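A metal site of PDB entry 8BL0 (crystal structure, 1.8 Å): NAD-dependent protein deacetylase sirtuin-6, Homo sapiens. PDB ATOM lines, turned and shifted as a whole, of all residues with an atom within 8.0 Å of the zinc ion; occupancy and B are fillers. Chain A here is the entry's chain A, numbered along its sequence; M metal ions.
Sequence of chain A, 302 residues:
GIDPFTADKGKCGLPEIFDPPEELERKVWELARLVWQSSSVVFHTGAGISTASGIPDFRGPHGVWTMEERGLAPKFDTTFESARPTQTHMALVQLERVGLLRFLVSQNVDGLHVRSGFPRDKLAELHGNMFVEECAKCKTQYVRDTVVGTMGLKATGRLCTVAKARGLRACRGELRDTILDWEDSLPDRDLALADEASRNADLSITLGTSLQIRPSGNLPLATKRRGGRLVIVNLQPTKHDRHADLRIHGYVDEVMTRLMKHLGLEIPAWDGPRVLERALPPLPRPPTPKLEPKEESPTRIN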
ATOM      1  N   GLU A 134     -17.034 -16.459  11.219  1.00  0.00           N
ATOM      2  CA  GLU A 134     -18.146 -17.120  10.506  1.00  0.00           C
ATOM      3  C   GLU A 134     -17.942 -16.938   9.001  1.00  0.00           C
ATOM      4  O   GLU A 134     -17.629 -15.807   8.597  1.00  0.00           O
ATOM      5  CB  GLU A 134     -19.477 -16.498  10.941  1.00  0.00           C
ATOM      6  CG  GLU A 134     -20.679 -17.115  10.250  1.00  0.00           C
ATOM      7  CD  GLU A 134     -22.012 -16.672  10.828  1.00  0.00           C
ATOM      8  OE1 GLU A 134     -22.223 -16.822  12.051  1.00  0.00           O
ATOM      9  OE2 GLU A 134     -22.843 -16.199  10.036  1.00  0.00           O
ATOM     10  N   CYS A 135     -18.115 -18.000   8.211  1.00  0.00           N
ATOM     11  CA  CYS A 135     -18.011 -17.956   6.727  1.00  0.00           C
ATOM     12  C   CYS A 135     -19.243 -17.211   6.190  1.00  0.00           C
ATOM     13  O   CYS A 135     -20.361 -17.576   6.570  1.00  0.00           O
ATOM     14  CB  CYS A 135     -17.905 -19.363   6.144  1.00  0.00           C
ATOM     15  SG  CYS A 135     -17.889 -19.480   4.325  1.00  0.00           S
ATOM     16  N   ALA A 136     -19.036 -16.205   5.345  1.00  0.00           N
ATOM     17  CA  ALA A 136     -20.138 -15.456   4.690  1.00  0.00           C
ATOM     18  C   ALA A 136     -20.960 -16.366   3.770  1.00  0.00           C
ATOM     19  O   ALA A 136     -22.153 -16.071   3.587  1.00  0.00           O
ATOM     20  CB  ALA A 136     -19.588 -14.281   3.939  1.00  0.00           C
ATOM     21  N   LYS A 137     -20.366 -17.447   3.235  1.00  0.00           N
ATOM     22  CA  LYS A 137     -21.048 -18.358   2.276  1.00  0.00           C
ATOM     23  C   LYS A 137     -21.822 -19.438   3.029  1.00  0.00           C
ATOM     24  O   LYS A 137     -23.063 -19.425   2.931  1.00  0.00           O
ATOM     25  CB  LYS A 137     -20.061 -19.046   1.330  1.00  0.00           C
ATOM     26  CG  LYS A 137     -19.450 -18.168   0.255  1.00  0.00           C
ATOM     27  CD  LYS A 137     -18.663 -18.977  -0.739  1.00  0.00           C
ATOM     28  CE  LYS A 137     -17.930 -18.144  -1.766  1.00  0.00           C
ATOM     29  NZ  LYS A 137     -17.022 -18.979  -2.592  1.00  0.00           N
ATOM     30  N   CYS A 138     -21.120 -20.334   3.728  1.00  0.00           N
ATOM     31  CA  CYS A 138     -21.724 -21.544   4.332  1.00  0.00           C
ATOM     32  C   CYS A 138     -22.154 -21.293   5.789  1.00  0.00           C
ATOM     33  O   CYS A 138     -22.788 -22.190   6.347  1.00  0.00           O
ATOM     34  CB  CYS A 138     -20.810 -22.758   4.193  1.00  0.00           C
ATOM     35  SG  CYS A 138     -19.253 -22.680   5.133  1.00  0.00           S
ATOM     36  N   LYS A 139     -21.832 -20.132   6.369  1.00  0.00           N
ATOM     37  CA  LYS A 139     -22.220 -19.739   7.761  1.00  0.00           C
ATOM     38  C   LYS A 139     -21.519 -20.633   8.793  1.00  0.00           C
ATOM     39  O   LYS A 139     -21.910 -20.565   9.969  1.00  0.00           O
ATOM     40  CB  LYS A 139     -23.743 -19.823   7.947  1.00  0.00           C
ATOM     41  CG  LYS A 139     -24.551 -19.049   6.913  1.00  0.00           C
ATOM     42  CD  LYS A 139     -24.154 -17.600   6.802  1.00  0.00           C
ATOM     43  CE  LYS A 139     -24.882 -16.865   5.697  1.00  0.00           C
ATOM     44  NZ  LYS A 139     -24.492 -15.448   5.628  1.00  0.00           N
ATOM     45  N   THR A 140     -20.543 -21.447   8.388  1.00  0.00           N
ATOM     46  CA  THR A 140     -19.767 -22.285   9.344  1.00  0.00           C
ATOM     47  C   THR A 140     -18.969 -21.356  10.275  1.00  0.00           C
ATOM     48  O   THR A 140     -18.300 -20.451   9.767  1.00  0.00           O
ATOM     49  CB  THR A 140     -18.854 -23.298   8.638  1.00  0.00           C
ATOM     50  OG1 THR A 140     -19.687 -24.219   7.927  1.00  0.00           O
ATOM     51  CG2 THR A 140     -17.974 -24.057   9.604  1.00  0.00           C
ATOM     52  N   GLN A 141     -19.025 -21.620  11.577  1.00  0.00           N
ATOM     53  CA  GLN A 141     -18.331 -20.835  12.627  1.00  0.00           C
ATOM     54  C   GLN A 141     -17.052 -21.562  13.034  1.00  0.00           C
ATOM     55  O   GLN A 141     -17.015 -22.805  13.025  1.00  0.00           O
ATOM     56  CB  GLN A 141     -19.259 -20.605  13.830  1.00  0.00           C
ATOM     57  CG  GLN A 141     -20.496 -19.801  13.458  1.00  0.00           C
ATOM     58  CD  GLN A 141     -21.231 -19.251  14.650  1.00  0.00           C
ATOM     59  OE1 GLN A 141     -21.339 -19.903  15.691  1.00  0.00           O
ATOM     60  NE2 GLN A 141     -21.760 -18.041  14.523  1.00  0.00           N
ATOM     61  N   TYR A 142     -16.005 -20.796  13.309  1.00  0.00           N
ATOM     62  CA  TYR A 142     -14.693 -21.278  13.787  1.00  0.00           C
ATOM     63  C   TYR A 142     -14.448 -20.602  15.129  1.00  0.00           C
ATOM     64  O   TYR A 142     -14.529 -19.366  15.188  1.00  0.00           O
ATOM     65  CB  TYR A 142     -13.593 -20.943  12.780  1.00  0.00           C
ATOM     66  CG  TYR A 142     -13.788 -21.576  11.422  1.00  0.00           C
ATOM     67  CD1 TYR A 142     -14.696 -21.056  10.514  1.00  0.00           C
ATOM     68  CD2 TYR A 142     -13.047 -22.688  11.043  1.00  0.00           C
ATOM     69  CE1 TYR A 142     -14.881 -21.628   9.274  1.00  0.00           C
ATOM     70  CE2 TYR A 142     -13.224 -23.277   9.795  1.00  0.00           C
ATOM     71  CZ  TYR A 142     -14.145 -22.745   8.901  1.00  0.00           C
ATOM     72  OH  TYR A 142     -14.321 -23.302   7.665  1.00  0.00           O
ATOM     73  N   LEU A 159      -9.834 -17.669   5.025  1.00  0.00           N
ATOM     74  CA  LEU A 159     -10.849 -18.319   4.142  1.00  0.00           C
ATOM     75  C   LEU A 159     -11.359 -19.595   4.784  1.00  0.00           C
ATOM     76  O   LEU A 159     -10.619 -20.223   5.561  1.00  0.00           O
ATOM     77  CB  LEU A 159     -10.236 -18.641   2.776  1.00  0.00           C
ATOM     78  CG  LEU A 159      -9.828 -17.431   1.923  1.00  0.00           C
ATOM     79  CD1 LEU A 159      -9.427 -17.885   0.523  1.00  0.00           C
ATOM     80  CD2 LEU A 159     -10.943 -16.403   1.857  1.00  0.00           C
ATOM     81  N   CYS A 160     -12.567 -19.999   4.394  1.00  0.00           N
ATOM     82  CA  CYS A 160     -13.263 -21.195   4.890  1.00  0.00           C
ATOM     83  C   CYS A 160     -12.547 -22.470   4.421  1.00  0.00           C
ATOM     84  O   CYS A 160     -12.125 -22.504   3.252  1.00  0.00           O
ATOM     85  CB  CYS A 160     -14.698 -21.200   4.393  1.00  0.00           C
ATOM     86  SG  CYS A 160     -15.715 -22.446   5.211  1.00  0.00           S
ATOM     87  N   THR A 161     -12.431 -23.466   5.293  1.00  0.00           N
ATOM     88  CA  THR A 161     -11.697 -24.730   5.044  1.00  0.00           C
ATOM     89  C   THR A 161     -12.675 -25.907   5.009  1.00  0.00           C
ATOM     90  O   THR A 161     -12.214 -27.056   5.025  1.00  0.00           O
ATOM     91  CB  THR A 161     -10.614 -24.941   6.113  1.00  0.00           C
ATOM     92  OG1 THR A 161     -11.264 -25.170   7.372  1.00  0.00           O
ATOM     93  CG2 THR A 161      -9.661 -23.776   6.208  1.00  0.00           C
ATOM     94  N   VAL A 162     -13.983 -25.651   4.990  1.00  0.00           N
ATOM     95  CA  VAL A 162     -15.001 -26.727   4.838  1.00  0.00           C
ATOM     96  C   VAL A 162     -14.856 -27.319   3.424  1.00  0.00           C
ATOM     97  O   VAL A 162     -14.623 -26.533   2.484  1.00  0.00           O
ATOM     98  CB  VAL A 162     -16.428 -26.235   5.138  1.00  0.00           C
ATOM     99  CG1 VAL A 162     -17.490 -27.233   4.695  1.00  0.00           C
ATOM    100  CG2 VAL A 162     -16.600 -25.917   6.613  1.00  0.00           C
ATOM    101  N   ALA A 163     -14.973 -28.650   3.312  1.00  0.00           N
ATOM    102  CA  ALA A 163     -14.690 -29.452   2.099  1.00  0.00           C
ATOM    103  C   ALA A 163     -15.523 -28.943   0.911  1.00  0.00           C
ATOM    104  O   ALA A 163     -16.754 -29.067   0.983  1.00  0.00           O
ATOM    105  CB  ALA A 163     -14.965 -30.913   2.376  1.00  0.00           C
ATOM    106  N   CYS A 171     -14.752 -24.612   0.177  1.00  0.00           N
ATOM    107  CA  CYS A 171     -15.703 -23.468   0.186  1.00  0.00           C
ATOM    108  C   CYS A 171     -14.929 -22.173  -0.062  1.00  0.00           C
ATOM    109  O   CYS A 171     -15.405 -21.325  -0.844  1.00  0.00           O
ATOM    110  CB  CYS A 171     -16.464 -23.396   1.505  1.00  0.00           C
ATOM    111  SG  CYS A 171     -17.348 -21.830   1.738  1.00  0.00           S
ATOM    112  N   ARG A 172     -13.785 -22.012   0.611  1.00  0.00           N
ATOM    113  CA  ARG A 172     -12.903 -20.830   0.496  1.00  0.00           C
ATOM    114  C   ARG A 172     -13.740 -19.548   0.617  1.00  0.00           C
ATOM    115  O   ARG A 172     -13.310 -18.517   0.077  1.00  0.00           O
ATOM    116  CB  ARG A 172     -12.104 -20.901  -0.806  1.00  0.00           C
ATOM    117  CG  ARG A 172     -11.523 -22.272  -1.113  1.00  0.00           C
ATOM    118  CD  ARG A 172     -10.239 -22.261  -1.928  1.00  0.00           C
ATOM    119  NE  ARG A 172     -10.093 -21.025  -2.715  1.00  0.00           N
ATOM    120  CZ  ARG A 172      -9.151 -20.103  -2.535  1.00  0.00           C
ATOM    121  NH1 ARG A 172      -8.220 -20.256  -1.604  1.00  0.00           N
ATOM    122  NH2 ARG A 172      -9.135 -19.022  -3.294  1.00  0.00           N
ATOM    123  N   GLY A 173     -14.862 -19.587   1.343  1.00  0.00           N
ATOM    124  CA  GLY A 173     -15.673 -18.393   1.672  1.00  0.00           C
ATOM    125  C   GLY A 173     -14.898 -17.397   2.531  1.00  0.00           C
ATOM    126  O   GLY A 173     -13.916 -17.809   3.207  1.00  0.00           O
ATOM    127  N   GLU A 174     -15.312 -16.134   2.494  1.00  0.00           N
ATOM    128  CA  GLU A 174     -14.739 -15.025   3.311  1.00  0.00           C
ATOM    129  C   GLU A 174     -15.119 -15.246   4.794  1.00  0.00           C
ATOM    130  O   GLU A 174     -16.333 -15.224   5.103  1.00  0.00           O
ATOM    131  CB  GLU A 174     -15.259 -13.683   2.766  1.00  0.00           C
ATOM    132  CG  GLU A 174     -14.658 -12.451   3.432  1.00  0.00           C
ATOM    133  CD  GLU A 174     -15.053 -11.128   2.793  1.00  0.00           C
ATOM    134  OE1 GLU A 174     -14.413 -10.761   1.787  1.00  0.00           O
ATOM    135  OE2 GLU A 174     -15.991 -10.461   3.308  1.00  0.00           O
ATOM    136  N   LEU A 175     -14.141 -15.482   5.667  1.00  0.00           N
ATOM    137  CA  LEU A 175     -14.380 -15.506   7.149  1.00  0.00           C
ATOM    138  C   LEU A 175     -14.533 -14.066   7.630  1.00  0.00           C
ATOM    139  O   LEU A 175     -13.707 -13.212   7.222  1.00  0.00           O
ATOM    140  CB  LEU A 175     -13.240 -16.238   7.864  1.00  0.00           C
ATOM    141  CG  LEU A 175     -13.086 -17.713   7.522  1.00  0.00           C
ATOM    142  CD1 LEU A 175     -12.297 -18.445   8.604  1.00  0.00           C
ATOM    143  CD2 LEU A 175     -14.436 -18.381   7.322  1.00  0.00           C
HETATM  144 ZN    ZN M   1     -17.640 -21.739   4.130  1.00  0.00          ZN
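OG1 of Thr 140 lies close to SG of Cys 138, at 3.2 Å.
The backbone NH (N) of Lys 137 sits close to the side-chain sulfur (SG) of Cys 135 (3.4 Å).
The side-chain sulfur of Cys 160 sits close to the backbone NH of Val 162.
SG of Cys 160 lies close to OH of Tyr 142, 2.9 Å away.
O of Cys 160 lies within hydrogen-bond range of N of Arg 172 (3.2 Å).
SG of Cys 171 lies close to N of Gly 173 (3.4 Å).
The backbone carbonyl oxygen of Cys 171 lies within hydrogen-bond range of the side-chain amino group of Lys 137.
The backbone NH (N) of Cys 171 is in hydrogen-bond range of the backbone carbonyl oxygen (O) of Val 162 (3.0 Å).
Within 4 Å of the zinc ion: Cys 135, Cys 138, Cys 160 and Cys 171.
The nearest printed residue that does not touch the zinc ion is Gly 173 (4.5 Å).
SG of Cys 138 binds the zinc ion (2.1 Å).
The zinc ion is bound by SG of Cys 135.
The side-chain sulfur (SG) of Cys 160 binds the zinc ion (2.3 Å).
SG of Cys 171 binds the zinc ion (2.4 Å).
The zinc ion has four donor atoms within binding distance.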
